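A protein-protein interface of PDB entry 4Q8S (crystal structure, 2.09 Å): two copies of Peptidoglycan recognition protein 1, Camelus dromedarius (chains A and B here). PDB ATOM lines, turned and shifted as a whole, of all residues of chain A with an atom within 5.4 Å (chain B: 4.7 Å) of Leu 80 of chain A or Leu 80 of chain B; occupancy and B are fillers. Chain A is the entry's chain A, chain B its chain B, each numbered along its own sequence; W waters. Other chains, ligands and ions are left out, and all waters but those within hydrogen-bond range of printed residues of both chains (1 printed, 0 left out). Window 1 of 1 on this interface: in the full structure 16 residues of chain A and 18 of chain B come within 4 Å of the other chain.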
ATOM      1  N   VAL A  10     -12.483 -19.964 -34.765  1.00  0.00           N
ATOM      2  CA  VAL A  10     -13.862 -19.641 -35.057  1.00  0.00           C
ATOM      3  C   VAL A  10     -13.755 -18.461 -36.013  1.00  0.00           C
ATOM      4  O   VAL A  10     -13.381 -17.357 -35.609  1.00  0.00           O
ATOM      5  CB  VAL A  10     -14.620 -19.224 -33.779  1.00  0.00           C
ATOM      6  CG1 VAL A  10     -16.056 -18.936 -34.110  1.00  0.00           C
ATOM      7  CG2 VAL A  10     -14.528 -20.326 -32.733  1.00  0.00           C
ATOM      8  N   PRO A  46     -19.188 -21.743 -26.342  1.00  0.00           N
ATOM      9  CA  PRO A  46     -19.060 -21.110 -27.655  1.00  0.00           C
ATOM     10  C   PRO A  46     -20.158 -20.074 -27.866  1.00  0.00           C
ATOM     11  O   PRO A  46     -19.967 -19.075 -28.556  1.00  0.00           O
ATOM     12  CB  PRO A  46     -19.135 -22.285 -28.640  1.00  0.00           C
ATOM     13  CG  PRO A  46     -19.459 -23.513 -27.798  1.00  0.00           C
ATOM     14  CD  PRO A  46     -18.997 -23.201 -26.413  1.00  0.00           C
ATOM     15  N   LEU A  74      -8.670 -13.616 -30.449  1.00  0.00           N
ATOM     16  CA  LEU A  74      -9.146 -13.575 -29.080  1.00  0.00           C
ATOM     17  C   LEU A  74      -9.241 -15.019 -28.595  1.00  0.00           C
ATOM     18  O   LEU A  74      -9.474 -15.937 -29.388  1.00  0.00           O
ATOM     19  CB  LEU A  74     -10.515 -12.896 -28.992  1.00  0.00           C
ATOM     20  CG  LEU A  74     -10.616 -11.466 -29.519  1.00  0.00           C
ATOM     21  CD1 LEU A  74     -11.042 -11.524 -30.969  1.00  0.00           C
ATOM     22  CD2 LEU A  74     -11.613 -10.665 -28.712  1.00  0.00           C
ATOM     23  N   ILE A  75      -9.068 -15.213 -27.291  1.00  0.00           N
ATOM     24  CA  ILE A  75      -9.114 -16.535 -26.688  1.00  0.00           C
ATOM     25  C   ILE A  75     -10.280 -16.664 -25.715  1.00  0.00           C
ATOM     26  O   ILE A  75     -10.421 -15.867 -24.794  1.00  0.00           O
ATOM     27  CB  ILE A  75      -7.814 -16.829 -25.910  1.00  0.00           C
ATOM     28  CG1 ILE A  75      -6.591 -16.540 -26.791  1.00  0.00           C
ATOM     29  CG2 ILE A  75      -7.843 -18.260 -25.387  1.00  0.00           C
ATOM     30  CD1 ILE A  75      -6.569 -17.264 -28.125  1.00  0.00           C
ATOM     31  N   GLY A  76     -11.117 -17.674 -25.909  1.00  0.00           N
ATOM     32  CA  GLY A  76     -12.238 -17.858 -25.005  1.00  0.00           C
ATOM     33  C   GLY A  76     -11.969 -18.880 -23.911  1.00  0.00           C
ATOM     34  O   GLY A  76     -11.184 -19.803 -24.099  1.00  0.00           O
ATOM     35  N   ASP A  78     -13.730 -20.948 -23.251  1.00  0.00           N
ATOM     36  CA  ASP A  78     -14.455 -22.089 -23.767  1.00  0.00           C
ATOM     37  C   ASP A  78     -13.428 -22.959 -24.497  1.00  0.00           C
ATOM     38  O   ASP A  78     -13.725 -24.071 -24.937  1.00  0.00           O
ATOM     39  CB  ASP A  78     -15.564 -21.611 -24.707  1.00  0.00           C
ATOM     40  CG  ASP A  78     -15.029 -20.900 -25.942  1.00  0.00           C
ATOM     41  OD1 ASP A  78     -13.856 -20.472 -25.944  1.00  0.00           O
ATOM     42  OD2 ASP A  78     -15.800 -20.756 -26.918  1.00  0.00           O
ATOM     43  N   GLY A  79     -12.212 -22.425 -24.603  1.00  0.00           N
ATOM     44  CA  GLY A  79     -11.126 -23.139 -25.244  1.00  0.00           C
ATOM     45  C   GLY A  79     -11.032 -22.952 -26.742  1.00  0.00           C
ATOM     46  O   GLY A  79     -10.323 -23.693 -27.413  1.00  0.00           O
ATOM     47  N   LEU A  80     -11.754 -21.982 -27.284  1.00  0.00           N
ATOM     48  CA  LEU A  80     -11.688 -21.748 -28.713  1.00  0.00           C
ATOM     49  C   LEU A  80     -10.972 -20.437 -29.022  1.00  0.00           C
ATOM     50  O   LEU A  80     -10.901 -19.534 -28.192  1.00  0.00           O
ATOM     51  CB  LEU A  80     -13.091 -21.737 -29.332  1.00  0.00           C
ATOM     52  CG  LEU A  80     -13.971 -22.977 -29.099  1.00  0.00           C
ATOM     53  CD1 LEU A  80     -15.271 -22.797 -29.883  1.00  0.00           C
ATOM     54  CD2 LEU A  80     -13.261 -24.248 -29.542  1.00  0.00           C
ATOM     55  N   VAL A  81     -10.420 -20.356 -30.222  1.00  0.00           N
ATOM     56  CA  VAL A  81      -9.734 -19.162 -30.677  1.00  0.00           C
ATOM     57  C   VAL A  81     -10.703 -18.437 -31.593  1.00  0.00           C
ATOM     58  O   VAL A  81     -11.328 -19.055 -32.456  1.00  0.00           O
ATOM     59  CB  VAL A  81      -8.480 -19.516 -31.474  1.00  0.00           C
ATOM     60  CG1 VAL A  81      -7.891 -18.271 -32.093  1.00  0.00           C
ATOM     61  CG2 VAL A  81      -7.470 -20.182 -30.562  1.00  0.00           C
ATOM     62  N   TYR A  82     -10.856 -17.140 -31.385  1.00  0.00           N
ATOM     63  CA  TYR A  82     -11.755 -16.369 -32.218  1.00  0.00           C
ATOM     64  C   TYR A  82     -10.921 -15.476 -33.107  1.00  0.00           C
ATOM     65  O   TYR A  82     -10.039 -14.766 -32.640  1.00  0.00           O
ATOM     66  CB  TYR A  82     -12.716 -15.560 -31.346  1.00  0.00           C
ATOM     67  CG  TYR A  82     -13.708 -16.445 -30.627  1.00  0.00           C
ATOM     68  CD1 TYR A  82     -15.009 -16.619 -31.117  1.00  0.00           C
ATOM     69  CD2 TYR A  82     -13.319 -17.185 -29.505  1.00  0.00           C
ATOM     70  CE1 TYR A  82     -15.892 -17.511 -30.509  1.00  0.00           C
ATOM     71  CE2 TYR A  82     -14.191 -18.079 -28.894  1.00  0.00           C
ATOM     72  CZ  TYR A  82     -15.473 -18.240 -29.403  1.00  0.00           C
ATOM     73  OH  TYR A  82     -16.318 -19.155 -28.826  1.00  0.00           O
ATOM     74  N   ARG A 119      -7.575 -25.102 -21.028  1.00  0.00           N
ATOM     75  CA  ARG A 119      -7.959 -25.138 -22.437  1.00  0.00           C
ATOM     76  C   ARG A 119      -7.765 -23.804 -23.154  1.00  0.00           C
ATOM     77  O   ARG A 119      -7.496 -23.772 -24.353  1.00  0.00           O
ATOM     78  CB  ARG A 119      -9.407 -25.612 -22.591  1.00  0.00           C
ATOM     79  CG  ARG A 119     -10.434 -24.697 -21.959  1.00  0.00           C
ATOM     80  CD  ARG A 119     -11.838 -25.271 -22.007  1.00  0.00           C
ATOM     81  NE  ARG A 119     -12.664 -24.580 -21.026  1.00  0.00           N
ATOM     82  CZ  ARG A 119     -12.886 -25.004 -19.787  1.00  0.00           C
ATOM     83  NH1 ARG A 119     -12.363 -26.144 -19.361  1.00  0.00           N
ATOM     84  NH2 ARG A 119     -13.591 -24.251 -18.957  1.00  0.00           N
ATOM     85  N   ALA A 123      -5.296 -23.315 -26.127  1.00  0.00           N
ATOM     86  CA  ALA A 123      -5.782 -22.734 -27.375  1.00  0.00           C
ATOM     87  C   ALA A 123      -4.779 -21.688 -27.876  1.00  0.00           C
ATOM     88  O   ALA A 123      -4.436 -21.652 -29.050  1.00  0.00           O
ATOM     89  CB  ALA A 123      -7.149 -22.095 -27.164  1.00  0.00           C
ATOM     90  N   VAL B  10      -8.285 -32.018 -25.078  1.00  0.00           N
ATOM     91  CA  VAL B  10      -8.505 -32.030 -23.638  1.00  0.00           C
ATOM     92  C   VAL B  10      -7.905 -33.358 -23.198  1.00  0.00           C
ATOM     93  O   VAL B  10      -8.316 -34.413 -23.672  1.00  0.00           O
ATOM     94  CB  VAL B  10     -10.001 -32.041 -23.271  1.00  0.00           C
ATOM     95  CG1 VAL B  10     -10.156 -32.045 -21.756  1.00  0.00           C
ATOM     96  CG2 VAL B  10     -10.700 -30.845 -23.891  1.00  0.00           C
ATOM     97  N   PRO B  46     -17.850 -27.228 -22.504  1.00  0.00           N
ATOM     98  CA  PRO B  46     -16.750 -27.987 -21.909  1.00  0.00           C
ATOM     99  C   PRO B  46     -17.170 -28.792 -20.693  1.00  0.00           C
ATOM    100  O   PRO B  46     -16.747 -29.930 -20.537  1.00  0.00           O
ATOM    101  CB  PRO B  46     -15.734 -26.905 -21.585  1.00  0.00           C
ATOM    102  CG  PRO B  46     -15.926 -25.964 -22.735  1.00  0.00           C
ATOM    103  CD  PRO B  46     -17.429 -25.846 -22.783  1.00  0.00           C
ATOM    104  N   LEU B  74     -12.644 -38.386 -28.898  1.00  0.00           N
ATOM    105  CA  LEU B  74     -14.060 -38.050 -28.936  1.00  0.00           C
ATOM    106  C   LEU B  74     -14.174 -36.568 -29.317  1.00  0.00           C
ATOM    107  O   LEU B  74     -13.309 -35.762 -28.958  1.00  0.00           O
ATOM    108  CB  LEU B  74     -14.733 -38.320 -27.582  1.00  0.00           C
ATOM    109  CG  LEU B  74     -14.788 -39.789 -27.129  1.00  0.00           C
ATOM    110  CD1 LEU B  74     -13.542 -40.107 -26.328  1.00  0.00           C
ATOM    111  CD2 LEU B  74     -16.036 -40.052 -26.275  1.00  0.00           C
ATOM    112  N   ILE B  75     -15.234 -36.228 -30.050  1.00  0.00           N
ATOM    113  CA  ILE B  75     -15.466 -34.862 -30.504  1.00  0.00           C
ATOM    114  C   ILE B  75     -16.736 -34.256 -29.932  1.00  0.00           C
ATOM    115  O   ILE B  75     -17.836 -34.719 -30.229  1.00  0.00           O
ATOM    116  CB  ILE B  75     -15.616 -34.777 -32.033  1.00  0.00           C
ATOM    117  CG1 ILE B  75     -14.503 -35.565 -32.724  1.00  0.00           C
ATOM    118  CG2 ILE B  75     -15.599 -33.317 -32.462  1.00  0.00           C
ATOM    119  CD1 ILE B  75     -13.102 -35.060 -32.427  1.00  0.00           C
ATOM    120  N   GLY B  76     -16.588 -33.203 -29.139  1.00  0.00           N
ATOM    121  CA  GLY B  76     -17.753 -32.574 -28.565  1.00  0.00           C
ATOM    122  C   GLY B  76     -18.285 -31.448 -29.426  1.00  0.00           C
ATOM    123  O   GLY B  76     -17.548 -30.828 -30.208  1.00  0.00           O
ATOM    124  N   ASP B  78     -18.863 -28.831 -28.445  1.00  0.00           N
ATOM    125  CA  ASP B  78     -18.330 -27.633 -27.813  1.00  0.00           C
ATOM    126  C   ASP B  78     -17.132 -27.185 -28.641  1.00  0.00           C
ATOM    127  O   ASP B  78     -16.512 -26.161 -28.374  1.00  0.00           O
ATOM    128  CB  ASP B  78     -17.931 -27.924 -26.359  1.00  0.00           C
ATOM    129  CG  ASP B  78     -16.906 -29.022 -26.241  1.00  0.00           C
ATOM    130  OD1 ASP B  78     -16.622 -29.692 -27.243  1.00  0.00           O
ATOM    131  OD2 ASP B  78     -16.378 -29.226 -25.136  1.00  0.00           O
ATOM    132  N   GLY B  79     -16.830 -27.960 -29.672  1.00  0.00           N
ATOM    133  CA  GLY B  79     -15.725 -27.625 -30.542  1.00  0.00           C
ATOM    134  C   GLY B  79     -14.403 -28.181 -30.067  1.00  0.00           C
ATOM    135  O   GLY B  79     -13.370 -27.834 -30.613  1.00  0.00           O
ATOM    136  N   LEU B  80     -14.422 -29.051 -29.065  1.00  0.00           N
ATOM    137  CA  LEU B  80     -13.185 -29.621 -28.546  1.00  0.00           C
ATOM    138  C   LEU B  80     -13.020 -31.118 -28.814  1.00  0.00           C
ATOM    139  O   LEU B  80     -13.992 -31.842 -29.070  1.00  0.00           O
ATOM    140  CB  LEU B  80     -13.088 -29.376 -27.038  1.00  0.00           C
ATOM    141  CG  LEU B  80     -13.243 -27.939 -26.525  1.00  0.00           C
ATOM    142  CD1 LEU B  80     -13.183 -27.964 -25.007  1.00  0.00           C
ATOM    143  CD2 LEU B  80     -12.148 -27.044 -27.091  1.00  0.00           C
ATOM    144  N   VAL B  81     -11.766 -31.560 -28.770  1.00  0.00           N
ATOM    145  CA  VAL B  81     -11.414 -32.955 -28.955  1.00  0.00           C
ATOM    146  C   VAL B  81     -11.002 -33.462 -27.587  1.00  0.00           C
ATOM    147  O   VAL B  81     -10.228 -32.813 -26.883  1.00  0.00           O
ATOM    148  CB  VAL B  81     -10.234 -33.133 -29.913  1.00  0.00           C
ATOM    149  CG1 VAL B  81      -9.822 -34.605 -29.955  1.00  0.00           C
ATOM    150  CG2 VAL B  81     -10.609 -32.652 -31.298  1.00  0.00           C
ATOM    151  N   TYR B  82     -11.534 -34.621 -27.216  1.00  0.00           N
ATOM    152  CA  TYR B  82     -11.250 -35.235 -25.922  1.00  0.00           C
ATOM    153  C   TYR B  82     -10.346 -36.417 -26.126  1.00  0.00           C
ATOM    154  O   TYR B  82     -10.595 -37.244 -26.996  1.00  0.00           O
ATOM    155  CB  TYR B  82     -12.558 -35.672 -25.261  1.00  0.00           C
ATOM    156  CG  TYR B  82     -13.366 -34.484 -24.824  1.00  0.00           C
ATOM    157  CD1 TYR B  82     -13.347 -34.065 -23.500  1.00  0.00           C
ATOM    158  CD2 TYR B  82     -14.033 -33.692 -25.763  1.00  0.00           C
ATOM    159  CE1 TYR B  82     -13.956 -32.889 -23.118  1.00  0.00           C
ATOM    160  CE2 TYR B  82     -14.646 -32.509 -25.393  1.00  0.00           C
ATOM    161  CZ  TYR B  82     -14.601 -32.109 -24.069  1.00  0.00           C
ATOM    162  OH  TYR B  82     -15.159 -30.909 -23.699  1.00  0.00           O
ATOM    163  N   ARG B 119     -17.814 -26.123 -35.811  1.00  0.00           N
ATOM    164  CA  ARG B 119     -16.658 -26.172 -34.926  1.00  0.00           C
ATOM    165  C   ARG B 119     -16.315 -27.587 -34.538  1.00  0.00           C
ATOM    166  O   ARG B 119     -15.148 -27.901 -34.339  1.00  0.00           O
ATOM    167  CB  ARG B 119     -16.888 -25.341 -33.666  1.00  0.00           C
ATOM    168  CG  ARG B 119     -18.009 -25.826 -32.781  1.00  0.00           C
ATOM    169  CD  ARG B 119     -18.173 -24.899 -31.597  1.00  0.00           C
ATOM    170  NE  ARG B 119     -19.487 -25.052 -30.994  1.00  0.00           N
ATOM    171  CZ  ARG B 119     -20.617 -24.597 -31.529  1.00  0.00           C
ATOM    172  NH1 ARG B 119     -20.602 -23.942 -32.683  1.00  0.00           N
ATOM    173  NH2 ARG B 119     -21.769 -24.826 -30.919  1.00  0.00           N
ATOM    174  N   ALA B 123     -12.669 -29.117 -35.313  1.00  0.00           N
ATOM    175  CA  ALA B 123     -11.813 -29.801 -34.357  1.00  0.00           C
ATOM    176  C   ALA B 123     -11.376 -31.152 -34.921  1.00  0.00           C
ATOM    177  O   ALA B 123     -10.272 -31.616 -34.649  1.00  0.00           O
ATOM    178  CB  ALA B 123     -12.562 -30.001 -33.036  1.00  0.00           C
HETATM  179  O   HOH W   1     -16.113 -24.948 -25.867  1.00  0.00           O
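Pro 46 of chain A touches Arg 119 of chain B, and with the chains exchanged Arg 119 of chain A touches Pro 46 of chain B. Asp 78 of chain A touches Pro 46 of chain B, but with the chains exchanged Pro 46 of chain A does not touch Asp 78 of chain B (4.004 Å). Asp 78 of chain A touches Leu 80 of chain B, and with the chains exchanged Leu 80 of chain A touches Asp 78 of chain B. Leu 80 of chain A touches Arg 119 of chain B, but with the chains exchanged Arg 119 of chain A does not touch Leu 80 of chain B (4.2 Å). 12 positions are printed for both chains.
Of the printed residues of chain B, Leu 80 of chain A touches Asp 78 (3.9 Å), Gly 79 (3.7 Å), Leu 80 (3.9 Å) and Arg 119 (3.97 Å). Printed residues of chain A within 4 Å of Pro 46 of chain B: Asp 78 and Arg 119. Ile 75 of chain B touches none of the printed residues of chain A. Printed residues of chain A within 4 Å of Asp 78 of chain B: Leu 80 (3.9 Å). Leu 80 of chain B touches just these residues of chain A: Asp 78, Gly 79 and Leu 80. The nearest residue of chain A that does not touch Leu 80 of chain B is Arg 119 of chain A (4.2 Å). The nearest printed residue of chain B that does not touch Pro 46 of chain A is Asp 78 of chain B (4.004 Å).
The backbone NH of Leu 80 of chain A lies within hydrogen-bond range of the side-chain carboxylate of Asp 78 of chain A (2.9 Å). The side-chain hydroxyl (OH) of Tyr 82 of chain A is in hydrogen-bond range of the side-chain carboxylate (OD2) of Asp 78 of chain A, at 2.5 Å. OD1 of Asp 78 of chain B lies within hydrogen-bond range of N of Leu 80 of chain B (2.9 Å). OH of Tyr 82 of chain B sits at hydrogen-bond distance from OD2 of Asp 78 of chain B, at 2.5 Å.
Water W1 lies within hydrogen-bond range of the backbone carbonyl oxygen (O) of Asp 78 of chain A (2.7 Å) and the backbone carbonyl oxygen (O) of Asp 78 of chain B (2.8 Å).
Printed residues of chain B that touch a printed residue of chain A: Pro 46, Asp 78, Gly 79, Leu 80 and Arg 119. Hydrophobic or aromatic side chains of chain B that line the printed part of chain A: Pro 46 and Leu 80. Of the 12 printed residues of chain A, 5 touch a printed residue of chain B. Printed residues of chain A that touch a printed residue of chain B: Pro 46, Asp 78, Gly 79, Leu 80 and Arg 119. Among the printed residues, no Asp or Glu carboxylate lies within 4 Å of a Lys or Arg side-chain nitrogen of the other chain.
Among the printed residues, pairs that only touch across the chains: Pro 46 of chain A with Arg 119 of chain B (3.5 Å), Asp 78 of chain A with Pro 46 of chain B (3.6 Å), Asp 78 of chain A with Leu 80 of chain B (3.9 Å), Gly 79 of chain A with Leu 80 of chain B (3.8 Å), Leu 80 of chain A with Asp 78 of chain B (3.9 Å), Leu 80 of chain A with Gly 79 of chain B (3.7 Å), Leu 80 of chain A with Leu 80 of chain B (3.9 Å), Leu 80 of chain A with Arg 119 of chain B (3.97 Å) and Arg 119 of chain A with Pro 46 of chain B (3.9 Å).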
